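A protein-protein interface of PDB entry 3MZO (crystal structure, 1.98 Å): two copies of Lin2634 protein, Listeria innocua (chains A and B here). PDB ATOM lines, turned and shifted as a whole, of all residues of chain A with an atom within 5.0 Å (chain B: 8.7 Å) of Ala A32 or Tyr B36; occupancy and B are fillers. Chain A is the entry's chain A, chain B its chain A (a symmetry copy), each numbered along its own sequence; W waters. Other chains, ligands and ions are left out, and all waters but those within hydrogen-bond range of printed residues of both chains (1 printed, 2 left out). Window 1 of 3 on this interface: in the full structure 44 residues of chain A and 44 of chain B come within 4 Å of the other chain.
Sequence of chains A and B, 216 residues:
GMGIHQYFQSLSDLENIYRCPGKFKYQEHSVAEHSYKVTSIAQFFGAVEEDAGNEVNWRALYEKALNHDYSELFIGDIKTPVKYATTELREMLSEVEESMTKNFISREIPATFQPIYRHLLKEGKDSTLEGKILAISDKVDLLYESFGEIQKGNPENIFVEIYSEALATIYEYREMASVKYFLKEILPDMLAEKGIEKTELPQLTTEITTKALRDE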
ATOM      1  N   LEU A  11      23.418 -15.305 -32.445  1.00  0.00           N
ATOM      2  CA  LEU A  11      23.269 -14.315 -31.401  1.00  0.00           C
ATOM      3  C   LEU A  11      23.651 -12.908 -31.857  1.00  0.00           C
ATOM      4  O   LEU A  11      22.981 -11.932 -31.501  1.00  0.00           O
ATOM      5  CB  LEU A  11      24.048 -14.716 -30.130  1.00  0.00           C
ATOM      6  CG  LEU A  11      23.553 -16.027 -29.473  1.00  0.00           C
ATOM      7  CD1 LEU A  11      24.559 -16.467 -28.349  1.00  0.00           C
ATOM      8  CD2 LEU A  11      22.121 -15.997 -28.932  1.00  0.00           C
ATOM      9  N   LEU A  14      21.094 -10.756 -33.955  1.00  0.00           N
ATOM     10  CA  LEU A  14      20.108 -10.004 -33.217  1.00  0.00           C
ATOM     11  C   LEU A  14      20.559  -8.602 -32.912  1.00  0.00           C
ATOM     12  O   LEU A  14      19.741  -7.798 -32.488  1.00  0.00           O
ATOM     13  CB  LEU A  14      19.675 -10.725 -31.924  1.00  0.00           C
ATOM     14  CG  LEU A  14      18.710 -11.869 -32.220  1.00  0.00           C
ATOM     15  CD1 LEU A  14      18.714 -12.849 -31.126  1.00  0.00           C
ATOM     16  CD2 LEU A  14      17.291 -11.362 -32.509  1.00  0.00           C
ATOM     17  N   GLU A  15      21.829  -8.289 -33.165  1.00  0.00           N
ATOM     18  CA  GLU A  15      22.324  -6.914 -33.060  1.00  0.00           C
ATOM     19  C   GLU A  15      21.965  -6.105 -34.299  1.00  0.00           C
ATOM     20  O   GLU A  15      22.162  -4.891 -34.327  1.00  0.00           O
ATOM     21  CB  GLU A  15      23.853  -6.887 -32.915  1.00  0.00           C
ATOM     22  CG  GLU A  15      24.360  -7.726 -31.715  1.00  0.00           C
ATOM     23  CD  GLU A  15      25.862  -7.892 -31.689  1.00  0.00           C
ATOM     24  OE1 GLU A  15      26.595  -7.184 -32.398  1.00  0.00           O
ATOM     25  OE2 GLU A  15      26.328  -8.755 -30.949  1.00  0.00           O
ATOM     26  N   SER A  30      18.775  -2.448 -30.642  1.00  0.00           N
ATOM     27  CA  SER A  30      18.662  -3.762 -31.267  1.00  0.00           C
ATOM     28  C   SER A  30      17.809  -4.719 -30.428  1.00  0.00           C
ATOM     29  O   SER A  30      17.589  -4.501 -29.238  1.00  0.00           O
ATOM     30  CB  SER A  30      20.054  -4.387 -31.514  1.00  0.00           C
ATOM     31  OG  SER A  30      20.672  -4.765 -30.281  1.00  0.00           O
ATOM     32  N   VAL A  31      17.393  -5.820 -31.010  1.00  0.00           N
ATOM     33  CA  VAL A  31      16.634  -6.770 -30.257  1.00  0.00           C
ATOM     34  C   VAL A  31      17.530  -7.354 -29.163  1.00  0.00           C
ATOM     35  O   VAL A  31      17.064  -7.658 -28.088  1.00  0.00           O
ATOM     36  CB  VAL A  31      16.059  -7.880 -31.161  1.00  0.00           C
ATOM     37  CG1 VAL A  31      15.469  -8.986 -30.284  1.00  0.00           C
ATOM     38  CG2 VAL A  31      14.991  -7.281 -32.103  1.00  0.00           C
ATOM     39  N   ALA A  32      18.830  -7.519 -29.461  1.00  0.00           N
ATOM     40  CA  ALA A  32      19.802  -8.007 -28.481  1.00  0.00           C
ATOM     41  C   ALA A  32      19.868  -7.117 -27.252  1.00  0.00           C
ATOM     42  O   ALA A  32      19.830  -7.592 -26.095  1.00  0.00           O
ATOM     43  CB  ALA A  32      21.259  -8.189 -29.140  1.00  0.00           C
ATOM     44  N   GLU A  33      19.962  -5.820 -27.502  1.00  0.00           N
ATOM     45  CA  GLU A  33      19.975  -4.833 -26.427  1.00  0.00           C
ATOM     46  C   GLU A  33      18.693  -4.810 -25.586  1.00  0.00           C
ATOM     47  O   GLU A  33      18.765  -4.807 -24.357  1.00  0.00           O
ATOM     48  CB  GLU A  33      20.307  -3.440 -27.011  1.00  0.00           C
ATOM     49  CG  GLU A  33      21.731  -3.422 -27.505  1.00  0.00           C
ATOM     50  CD  GLU A  33      22.103  -2.255 -28.418  1.00  0.00           C
ATOM     51  OE1 GLU A  33      21.213  -1.667 -29.081  1.00  0.00           O
ATOM     52  OE2 GLU A  33      23.313  -1.949 -28.444  1.00  0.00           O
ATOM     53  N   HIS A  34      17.540  -4.831 -26.255  1.00  0.00           N
ATOM     54  CA  HIS A  34      16.230  -4.926 -25.590  1.00  0.00           C
ATOM     55  C   HIS A  34      16.197  -6.181 -24.690  1.00  0.00           C
ATOM     56  O   HIS A  34      15.710  -6.126 -23.581  1.00  0.00           O
ATOM     57  CB  HIS A  34      15.133  -5.024 -26.650  1.00  0.00           C
ATOM     58  CG  HIS A  34      13.800  -5.487 -26.133  1.00  0.00           C
ATOM     59  ND1 HIS A  34      12.973  -4.686 -25.368  1.00  0.00           N
ATOM     60  CD2 HIS A  34      13.137  -6.652 -26.306  1.00  0.00           C
ATOM     61  CE1 HIS A  34      11.861  -5.344 -25.097  1.00  0.00           C
ATOM     62  NE2 HIS A  34      11.929  -6.532 -25.667  1.00  0.00           N
ATOM     63  N   SER A  35      16.734  -7.296 -25.189  1.00  0.00           N
ATOM     64  CA  SER A  35      16.767  -8.521 -24.413  1.00  0.00           C
ATOM     65  C   SER A  35      17.629  -8.374 -23.160  1.00  0.00           C
ATOM     66  O   SER A  35      17.207  -8.790 -22.098  1.00  0.00           O
ATOM     67  CB  SER A  35      17.207  -9.710 -25.225  1.00  0.00           C
ATOM     68  OG  SER A  35      16.330  -9.868 -26.348  1.00  0.00           O
ATOM     69  N   TYR A  36      18.804  -7.788 -23.293  1.00  0.00           N
ATOM     70  CA  TYR A  36      19.669  -7.508 -22.141  1.00  0.00           C
ATOM     71  C   TYR A  36      18.899  -6.665 -21.118  1.00  0.00           C
ATOM     72  O   TYR A  36      18.915  -6.937 -19.916  1.00  0.00           O
ATOM     73  CB  TYR A  36      20.944  -6.782 -22.602  1.00  0.00           C
ATOM     74  CG  TYR A  36      21.683  -6.112 -21.446  1.00  0.00           C
ATOM     75  CD1 TYR A  36      22.398  -6.865 -20.518  1.00  0.00           C
ATOM     76  CD2 TYR A  36      21.586  -4.740 -21.261  1.00  0.00           C
ATOM     77  CE1 TYR A  36      23.022  -6.243 -19.418  1.00  0.00           C
ATOM     78  CE2 TYR A  36      22.213  -4.126 -20.225  1.00  0.00           C
ATOM     79  CZ  TYR A  36      22.924  -4.864 -19.297  1.00  0.00           C
ATOM     80  OH  TYR A  36      23.500  -4.165 -18.256  1.00  0.00           O
ATOM     81  N   LEU A  66      15.410 -13.570 -21.007  1.00  0.00           N
ATOM     82  CA  LEU A  66      16.515 -13.572 -21.960  1.00  0.00           C
ATOM     83  C   LEU A  66      16.138 -13.996 -23.377  1.00  0.00           C
ATOM     84  O   LEU A  66      16.639 -13.456 -24.369  1.00  0.00           O
ATOM     85  CB  LEU A  66      17.633 -14.474 -21.433  1.00  0.00           C
ATOM     86  CG  LEU A  66      18.926 -14.471 -22.234  1.00  0.00           C
ATOM     87  CD1 LEU A  66      19.636 -13.147 -21.979  1.00  0.00           C
ATOM     88  CD2 LEU A  66      19.803 -15.630 -21.864  1.00  0.00           C
ATOM     89  N   TYR A  70      14.130 -13.821 -29.194  1.00  0.00           N
ATOM     90  CA  TYR A  70      15.059 -14.503 -30.054  1.00  0.00           C
ATOM     91  C   TYR A  70      14.427 -14.789 -31.456  1.00  0.00           C
ATOM     92  O   TYR A  70      15.088 -14.644 -32.481  1.00  0.00           O
ATOM     93  CB  TYR A  70      15.540 -15.819 -29.386  1.00  0.00           C
ATOM     94  CG  TYR A  70      16.489 -16.578 -30.280  1.00  0.00           C
ATOM     95  CD1 TYR A  70      17.821 -16.165 -30.434  1.00  0.00           C
ATOM     96  CD2 TYR A  70      16.064 -17.661 -31.021  1.00  0.00           C
ATOM     97  CE1 TYR A  70      18.695 -16.844 -31.273  1.00  0.00           C
ATOM     98  CE2 TYR A  70      16.948 -18.347 -31.885  1.00  0.00           C
ATOM     99  CZ  TYR A  70      18.255 -17.931 -31.999  1.00  0.00           C
ATOM    100  OH  TYR A  70      19.108 -18.568 -32.881  1.00  0.00           O
ATOM    101  N   GLU B  15      24.411   0.554 -24.434  1.00  0.00           N
ATOM    102  CA  GLU B  15      24.314   0.395 -25.886  1.00  0.00           C
ATOM    103  C   GLU B  15      25.251   1.353 -26.608  1.00  0.00           C
ATOM    104  O   GLU B  15      25.421   1.259 -27.823  1.00  0.00           O
ATOM    105  CB  GLU B  15      22.888   0.682 -26.379  1.00  0.00           C
ATOM    106  CG  GLU B  15      21.819  -0.194 -25.677  1.00  0.00           C
ATOM    107  CD  GLU B  15      20.401   0.225 -25.985  1.00  0.00           C
ATOM    108  OE1 GLU B  15      20.154   1.001 -26.922  1.00  0.00           O
ATOM    109  OE2 GLU B  15      19.505  -0.221 -25.271  1.00  0.00           O
ATOM    110  N   GLN B  27      31.629  -5.398 -37.949  1.00  0.00           N
ATOM    111  CA  GLN B  27      30.433  -5.312 -37.076  1.00  0.00           C
ATOM    112  C   GLN B  27      30.870  -4.905 -35.664  1.00  0.00           C
ATOM    113  O   GLN B  27      31.619  -5.644 -35.032  1.00  0.00           O
ATOM    114  CB  GLN B  27      29.650  -6.663 -37.069  1.00  0.00           C
ATOM    115  CG  GLN B  27      28.305  -6.534 -36.257  1.00  0.00           C
ATOM    116  CD  GLN B  27      27.286  -7.671 -36.444  1.00  0.00           C
ATOM    117  OE1 GLN B  27      27.196  -8.285 -37.521  1.00  0.00           O
ATOM    118  NE2 GLN B  27      26.490  -7.941 -35.372  1.00  0.00           N
ATOM    119  N   HIS B  29      30.137  -4.202 -31.551  1.00  0.00           N
ATOM    120  CA  HIS B  29      29.247  -4.840 -30.583  1.00  0.00           C
ATOM    121  C   HIS B  29      29.217  -3.975 -29.362  1.00  0.00           C
ATOM    122  O   HIS B  29      30.258  -3.692 -28.833  1.00  0.00           O
ATOM    123  CB  HIS B  29      29.742  -6.262 -30.223  1.00  0.00           C
ATOM    124  CG  HIS B  29      30.028  -7.138 -31.400  1.00  0.00           C
ATOM    125  ND1 HIS B  29      29.039  -7.678 -32.196  1.00  0.00           N
ATOM    126  CD2 HIS B  29      31.207  -7.536 -31.946  1.00  0.00           C
ATOM    127  CE1 HIS B  29      29.594  -8.388 -33.164  1.00  0.00           C
ATOM    128  NE2 HIS B  29      30.911  -8.297 -33.049  1.00  0.00           N
ATOM    129  N   SER B  30      28.037  -3.540 -28.894  1.00  0.00           N
ATOM    130  CA  SER B  30      27.966  -2.788 -27.645  1.00  0.00           C
ATOM    131  C   SER B  30      28.212  -3.685 -26.428  1.00  0.00           C
ATOM    132  O   SER B  30      28.103  -4.908 -26.503  1.00  0.00           O
ATOM    133  CB  SER B  30      26.603  -2.074 -27.497  1.00  0.00           C
ATOM    134  OG  SER B  30      25.553  -3.016 -27.265  1.00  0.00           O
ATOM    135  N   VAL B  31      28.462  -3.090 -25.284  1.00  0.00           N
ATOM    136  CA  VAL B  31      28.652  -3.879 -24.106  1.00  0.00           C
ATOM    137  C   VAL B  31      27.335  -4.582 -23.772  1.00  0.00           C
ATOM    138  O   VAL B  31      27.340  -5.689 -23.283  1.00  0.00           O
ATOM    139  CB  VAL B  31      29.145  -3.022 -22.922  1.00  0.00           C
ATOM    140  CG1 VAL B  31      29.099  -3.859 -21.642  1.00  0.00           C
ATOM    141  CG2 VAL B  31      30.575  -2.513 -23.209  1.00  0.00           C
ATOM    142  N   ALA B  32      26.200  -3.911 -24.036  1.00  0.00           N
ATOM    143  CA  ALA B  32      24.876  -4.498 -23.823  1.00  0.00           C
ATOM    144  C   ALA B  32      24.684  -5.776 -24.622  1.00  0.00           C
ATOM    145  O   ALA B  32      24.226  -6.815 -24.098  1.00  0.00           O
ATOM    146  CB  ALA B  32      23.707  -3.439 -24.138  1.00  0.00           C
ATOM    147  N   GLU B  33      25.039  -5.699 -25.896  1.00  0.00           N
ATOM    148  CA  GLU B  33      24.970  -6.859 -26.779  1.00  0.00           C
ATOM    149  C   GLU B  33      25.879  -8.019 -26.358  1.00  0.00           C
ATOM    150  O   GLU B  33      25.433  -9.166 -26.319  1.00  0.00           O
ATOM    151  CB  GLU B  33      25.240  -6.414 -28.235  1.00  0.00           C
ATOM    152  CG  GLU B  33      24.105  -5.548 -28.721  1.00  0.00           C
ATOM    153  CD  GLU B  33      24.377  -4.747 -29.993  1.00  0.00           C
ATOM    154  OE1 GLU B  33      25.556  -4.452 -30.310  1.00  0.00           O
ATOM    155  OE2 GLU B  33      23.372  -4.427 -30.660  1.00  0.00           O
ATOM    156  N   HIS B  34      27.129  -7.704 -26.015  1.00  0.00           N
ATOM    157  CA  HIS B  34      28.086  -8.688 -25.483  1.00  0.00           C
ATOM    158  C   HIS B  34      27.484  -9.370 -24.234  1.00  0.00           C
ATOM    159  O   HIS B  34      27.598 -10.567 -24.076  1.00  0.00           O
ATOM    160  CB  HIS B  34      29.384  -7.976 -25.106  1.00  0.00           C
ATOM    161  CG  HIS B  34      30.304  -8.773 -24.225  1.00  0.00           C
ATOM    162  ND1 HIS B  34      31.042  -9.846 -24.687  1.00  0.00           N
ATOM    163  CD2 HIS B  34      30.634  -8.625 -22.922  1.00  0.00           C
ATOM    164  CE1 HIS B  34      31.784 -10.319 -23.702  1.00  0.00           C
ATOM    165  NE2 HIS B  34      31.566  -9.587 -22.627  1.00  0.00           N
ATOM    166  N   SER B  35      26.840  -8.584 -23.369  1.00  0.00           N
ATOM    167  CA  SER B  35      26.225  -9.135 -22.176  1.00  0.00           C
ATOM    168  C   SER B  35      25.095 -10.104 -22.516  1.00  0.00           C
ATOM    169  O   SER B  35      25.031 -11.170 -21.934  1.00  0.00           O
ATOM    170  CB  SER B  35      25.745  -8.068 -21.227  1.00  0.00           C
ATOM    171  OG  SER B  35      26.846  -7.225 -20.865  1.00  0.00           O
ATOM    172  N   TYR B  36      24.232  -9.734 -23.444  1.00  0.00           N
ATOM    173  CA  TYR B  36      23.168 -10.625 -23.918  1.00  0.00           C
ATOM    174  C   TYR B  36      23.785 -11.934 -24.425  1.00  0.00           C
ATOM    175  O   TYR B  36      23.321 -13.030 -24.107  1.00  0.00           O
ATOM    176  CB  TYR B  36      22.355  -9.936 -25.028  1.00  0.00           C
ATOM    177  CG  TYR B  36      21.513 -10.923 -25.832  1.00  0.00           C
ATOM    178  CD1 TYR B  36      20.364 -11.494 -25.290  1.00  0.00           C
ATOM    179  CD2 TYR B  36      21.928 -11.324 -27.094  1.00  0.00           C
ATOM    180  CE1 TYR B  36      19.630 -12.454 -26.016  1.00  0.00           C
ATOM    181  CE2 TYR B  36      21.208 -12.221 -27.816  1.00  0.00           C
ATOM    182  CZ  TYR B  36      20.067 -12.795 -27.287  1.00  0.00           C
ATOM    183  OH  TYR B  36      19.417 -13.723 -28.074  1.00  0.00           O
ATOM    184  N   LYS B  37      24.835 -11.809 -25.227  1.00  0.00           N
ATOM    185  CA  LYS B  37      25.440 -12.993 -25.837  1.00  0.00           C
ATOM    186  C   LYS B  37      26.143 -13.871 -24.795  1.00  0.00           C
ATOM    187  O   LYS B  37      25.982 -15.073 -24.803  1.00  0.00           O
ATOM    188  CB  LYS B  37      26.391 -12.594 -26.964  1.00  0.00           C
ATOM    189  CG  LYS B  37      25.667 -11.960 -28.179  1.00  0.00           C
ATOM    190  CD  LYS B  37      26.639 -11.618 -29.334  1.00  0.00           C
ATOM    191  CE  LYS B  37      27.619 -10.526 -28.933  1.00  0.00           C
ATOM    192  NZ  LYS B  37      28.475 -10.140 -30.115  1.00  0.00           N
ATOM    193  N   VAL B  38      26.867 -13.266 -23.866  1.00  0.00           N
ATOM    194  CA  VAL B  38      27.529 -14.054 -22.830  1.00  0.00           C
ATOM    195  C   VAL B  38      26.489 -14.823 -21.983  1.00  0.00           C
ATOM    196  O   VAL B  38      26.736 -15.967 -21.607  1.00  0.00           O
ATOM    197  CB  VAL B  38      28.514 -13.200 -21.965  1.00  0.00           C
ATOM    198  CG1 VAL B  38      29.064 -14.027 -20.709  1.00  0.00           C
ATOM    199  CG2 VAL B  38      29.675 -12.699 -22.830  1.00  0.00           C
ATOM    200  N   THR B  39      25.337 -14.206 -21.682  1.00  0.00           N
ATOM    201  CA  THR B  39      24.334 -14.851 -20.855  1.00  0.00           C
ATOM    202  C   THR B  39      23.700 -16.009 -21.638  1.00  0.00           C
ATOM    203  O   THR B  39      23.445 -17.078 -21.074  1.00  0.00           O
ATOM    204  CB  THR B  39      23.294 -13.820 -20.386  1.00  0.00           C
ATOM    205  OG1 THR B  39      23.978 -12.719 -19.801  1.00  0.00           O
ATOM    206  CG2 THR B  39      22.329 -14.374 -19.352  1.00  0.00           C
ATOM    207  N   SER B  40      23.510 -15.826 -22.948  1.00  0.00           N
ATOM    208  CA  SER B  40      22.952 -16.889 -23.785  1.00  0.00           C
ATOM    209  C   SER B  40      23.914 -18.092 -23.901  1.00  0.00           C
ATOM    210  O   SER B  40      23.475 -19.243 -23.883  1.00  0.00           O
ATOM    211  CB  SER B  40      22.575 -16.327 -25.178  1.00  0.00           C
ATOM    212  OG  SER B  40      21.568 -15.288 -25.056  1.00  0.00           O
ATOM    213  N   ILE B  41      25.202 -17.799 -24.015  1.00  0.00           N
ATOM    214  CA  ILE B  41      26.280 -18.817 -24.105  1.00  0.00           C
ATOM    215  C   ILE B  41      26.320 -19.546 -22.722  1.00  0.00           C
ATOM    216  O   ILE B  41      26.292 -20.757 -22.659  1.00  0.00           O
ATOM    217  CB  ILE B  41      27.658 -18.155 -24.455  1.00  0.00           C
ATOM    218  CG1 ILE B  41      27.693 -17.673 -25.914  1.00  0.00           C
ATOM    219  CG2 ILE B  41      28.877 -19.137 -24.185  1.00  0.00           C
ATOM    220  CD1 ILE B  41      28.791 -16.622 -26.260  1.00  0.00           C
ATOM    221  N   ALA B  42      26.338 -18.783 -21.631  1.00  0.00           N
ATOM    222  CA  ALA B  42      26.329 -19.356 -20.295  1.00  0.00           C
ATOM    223  C   ALA B  42      25.090 -20.252 -20.055  1.00  0.00           C
ATOM    224  O   ALA B  42      25.227 -21.316 -19.494  1.00  0.00           O
ATOM    225  CB  ALA B  42      26.433 -18.259 -19.227  1.00  0.00           C
ATOM    226  N   GLN B  43      23.918 -19.816 -20.511  1.00  0.00           N
ATOM    227  CA  GLN B  43      22.690 -20.570 -20.452  1.00  0.00           C
ATOM    228  C   GLN B  43      22.852 -21.936 -21.140  1.00  0.00           C
ATOM    229  O   GLN B  43      22.412 -22.986 -20.619  1.00  0.00           O
ATOM    230  CB  GLN B  43      21.577 -19.758 -21.129  1.00  0.00           C
ATOM    231  CG  GLN B  43      20.271 -20.481 -21.406  1.00  0.00           C
ATOM    232  CD  GLN B  43      19.227 -19.505 -21.931  1.00  0.00           C
ATOM    233  OE1 GLN B  43      18.447 -18.951 -21.158  1.00  0.00           O
ATOM    234  NE2 GLN B  43      19.251 -19.248 -23.240  1.00  0.00           N
ATOM    235  N   TYR B  62      23.194 -17.052 -14.110  1.00  0.00           N
ATOM    236  CA  TYR B  62      22.588 -15.983 -14.879  1.00  0.00           C
ATOM    237  C   TYR B  62      23.037 -14.626 -14.366  1.00  0.00           C
ATOM    238  O   TYR B  62      23.429 -13.773 -15.165  1.00  0.00           O
ATOM    239  CB  TYR B  62      21.061 -16.084 -14.865  1.00  0.00           C
ATOM    240  CG  TYR B  62      20.447 -17.023 -15.888  1.00  0.00           C
ATOM    241  CD1 TYR B  62      20.494 -16.738 -17.264  1.00  0.00           C
ATOM    242  CD2 TYR B  62      19.729 -18.140 -15.484  1.00  0.00           C
ATOM    243  CE1 TYR B  62      19.878 -17.565 -18.190  1.00  0.00           C
ATOM    244  CE2 TYR B  62      19.133 -18.993 -16.403  1.00  0.00           C
ATOM    245  CZ  TYR B  62      19.202 -18.717 -17.741  1.00  0.00           C
ATOM    246  OH  TYR B  62      18.580 -19.543 -18.657  1.00  0.00           O
ATOM    247  N   ALA B  65      26.710 -13.857 -15.418  1.00  0.00           N
ATOM    248  CA  ALA B  65      26.821 -13.608 -16.865  1.00  0.00           C
ATOM    249  C   ALA B  65      26.195 -12.263 -17.259  1.00  0.00           C
ATOM    250  O   ALA B  65      26.828 -11.416 -17.926  1.00  0.00           O
ATOM    251  CB  ALA B  65      26.179 -14.784 -17.656  1.00  0.00           C
ATOM    252  N   LEU B  66      24.987 -12.016 -16.781  1.00  0.00           N
ATOM    253  CA  LEU B  66      24.279 -10.802 -17.173  1.00  0.00           C
ATOM    254  C   LEU B  66      24.942  -9.502 -16.729  1.00  0.00           C
ATOM    255  O   LEU B  66      24.946  -8.498 -17.450  1.00  0.00           O
ATOM    256  CB  LEU B  66      22.847 -10.859 -16.637  1.00  0.00           C
ATOM    257  CG  LEU B  66      21.922  -9.736 -17.083  1.00  0.00           C
ATOM    258  CD1 LEU B  66      21.568  -9.972 -18.548  1.00  0.00           C
ATOM    259  CD2 LEU B  66      20.685  -9.675 -16.237  1.00  0.00           C
ATOM    260  N   ASN B  67      25.495  -9.502 -15.526  1.00  0.00           N
ATOM    261  CA  ASN B  67      25.988  -8.287 -14.920  1.00  0.00           C
ATOM    262  C   ASN B  67      27.505  -8.066 -14.966  1.00  0.00           C
ATOM    263  O   ASN B  67      27.976  -7.053 -14.508  1.00  0.00           O
ATOM    264  CB  ASN B  67      25.561  -8.250 -13.473  1.00  0.00           C
ATOM    265  CG  ASN B  67      24.075  -8.443 -13.319  1.00  0.00           C
ATOM    266  OD1 ASN B  67      23.299  -7.606 -13.755  1.00  0.00           O
ATOM    267  ND2 ASN B  67      23.677  -9.562 -12.739  1.00  0.00           N
ATOM    268  N   HIS B  68      28.249  -8.971 -15.562  1.00  0.00           N
ATOM    269  CA  HIS B  68      29.699  -8.917 -15.471  1.00  0.00           C
ATOM    270  C   HIS B  68      30.401  -7.707 -16.057  1.00  0.00           C
ATOM    271  O   HIS B  68      31.484  -7.421 -15.602  1.00  0.00           O
ATOM    272  CB  HIS B  68      30.328 -10.196 -16.018  1.00  0.00           C
ATOM    273  CG  HIS B  68      30.469 -10.220 -17.505  1.00  0.00           C
ATOM    274  ND1 HIS B  68      29.412 -10.477 -18.348  1.00  0.00           N
ATOM    275  CD2 HIS B  68      31.555 -10.061 -18.300  1.00  0.00           C
ATOM    276  CE1 HIS B  68      29.838 -10.462 -19.604  1.00  0.00           C
ATOM    277  NE2 HIS B  68      31.134 -10.224 -19.602  1.00  0.00           N
ATOM    278  N   ASP B  69      29.800  -7.003 -17.032  1.00  0.00           N
ATOM    279  CA  ASP B  69      30.405  -5.827 -17.639  1.00  0.00           C
ATOM    280  C   ASP B  69      29.604  -4.554 -17.469  1.00  0.00           C
ATOM    281  O   ASP B  69      29.933  -3.553 -18.072  1.00  0.00           O
ATOM    282  CB  ASP B  69      30.689  -6.052 -19.128  1.00  0.00           C
ATOM    283  CG  ASP B  69      31.962  -6.855 -19.385  1.00  0.00           C
ATOM    284  OD1 ASP B  69      32.744  -7.078 -18.477  1.00  0.00           O
ATOM    285  OD2 ASP B  69      32.203  -7.252 -20.527  1.00  0.00           O
ATOM    286  N   ASP B 141      32.483 -15.639 -26.269  1.00  0.00           N
ATOM    287  CA  ASP B 141      32.027 -14.473 -27.038  1.00  0.00           C
ATOM    288  C   ASP B 141      33.203 -13.740 -27.720  1.00  0.00           C
ATOM    289  O   ASP B 141      33.102 -13.334 -28.866  1.00  0.00           O
ATOM    290  CB  ASP B 141      31.277 -13.453 -26.205  1.00  0.00           C
ATOM    291  CG  ASP B 141      30.526 -12.420 -27.094  1.00  0.00           C
ATOM    292  OD1 ASP B 141      29.859 -12.834 -28.103  1.00  0.00           O
ATOM    293  OD2 ASP B 141      30.689 -11.200 -26.836  1.00  0.00           O
HETATM  294  O   HOH W   1      22.684  -5.874 -15.996  1.00  0.00           O
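The side-chain amide nitrogen (NE2) of Gln B27 lies within hydrogen-bond range of the side-chain carboxylate (OE1) of Glu A15 (3.1 Å). ND1 of His B29 is in hydrogen-bond range of OE1 of Glu A15 (2.5 Å). The side-chain carboxylate of Glu A15 is in salt-bridge range of the side-chain amino group of Lys B37, 2.7 Å away. The side-chain hydroxyl (OG) of Ser A30 lies within hydrogen-bond range of the side-chain carboxylate (OE2) of Glu B33. The side-chain carboxylate of Glu A33 sits at hydrogen-bond distance from the side-chain hydroxyl of Ser B30 (2.7 Å). The side-chain carboxylate of Glu B33 lies close to the side-chain carboxylate of Glu A33 (3.3 Å).
O of Leu A14 lies within hydrogen-bond range of N of Ala A32 (3.2 Å). NE2 of His B29 sits at hydrogen-bond distance from O of Gln B27, 3.4 Å away. OG of Ser B30 lies close to N of Ala B32. The backbone carbonyl oxygen (O) of Tyr B36 is in hydrogen-bond range of the side-chain hydroxyl (OG) of Ser B40 (3.0 Å). The side-chain amino group of Lys B37 lies within salt-bridge range of the side-chain carboxylate of Asp B141 (3.6 Å). N of Leu B66 sits at hydrogen-bond distance from OG1 of Thr B39 (3.3 Å).
CD1 of Leu A11 touches CB of Ser B40 (3.7 Å). Glu A15 touches Glu B33. Glu B33 touches Ala A32 (CG to CB, 3.9 Å). Glu A33 touches Glu B15. Ala B32 touches Glu A33 (CB to CG, 3.9 Å). Ala B32 touches Tyr A36. Tyr A36 touches Leu B66 (CE1 to O, 3.6 Å). Leu A66 touches Tyr B36 (O to CE1, 3.6 Å). Thr B39 touches Leu A66. Leu A66 touches Gln B43.
Of chain B, only Glu B33 (3.9 Å) and Tyr B36 (3.6 Å) come within 4 Å of Ala A32. Of chain A, only Leu A11, Leu A14, Ala A32, Ser A35, Leu A66 and Tyr A70 come within 4 Å of Tyr B36. Of the printed residues of chain B, Ser A35 touches Tyr B36 (3.6 Å). Of the printed residues of chain B, Tyr A70 touches Tyr B36. Printed residues of chain A within 4 Å of Ser B35: Tyr A36 (3.6 Å). Of the printed residues of chain B, Tyr A36 touches Ala B32, Ser B35 and Leu B66. Asp B69 touches none of the printed residues of chain A. The nearest residue of chain B that does not touch Ala A32 is Ala B32 (4.9 Å). The nearest printed residue of chain A that does not touch Lys B37 is Ala A32 (5.9 Å).
Hydrophobic or aromatic side chains of chain A within 4 Å of the printed part of chain B: Leu A11, Leu A14, Ala A32, Tyr A36, Leu A66 and Tyr A70. Of the 24 printed residues of chain B, 13 touch a printed residue of chain A. Printed residues of chain B that touch a printed residue of chain A: Glu B15, Gln B27, His B29, Ser B30, Ala B32, Glu B33, Ser B35, Tyr B36, Lys B37, Thr B39, Ser B40, Gln B43 and Leu B66. Among the printed residues, Asp or Glu carboxylates within 4 Å of a Lys or Arg side-chain nitrogen of the other chain: Glu A15 with Lys B37 (2.7 Å).
Ser A30 touches Glu B33, and with the chains exchanged Glu A33 touches Ser B30. Ala A32 touches Tyr B36, and with the chains exchanged Tyr A36 touches Ala B32. Ser A35 touches Tyr B36, and with the chains exchanged Tyr A36 touches Ser B35. Tyr A36 touches Leu B66, and with the chains exchanged Leu A66 touches Tyr B36.
Water W1 bridges the side-chain amide oxygen of Asn B67 (2.9 Å) and the side-chain hydroxyl of Tyr A36 (2.9 Å).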
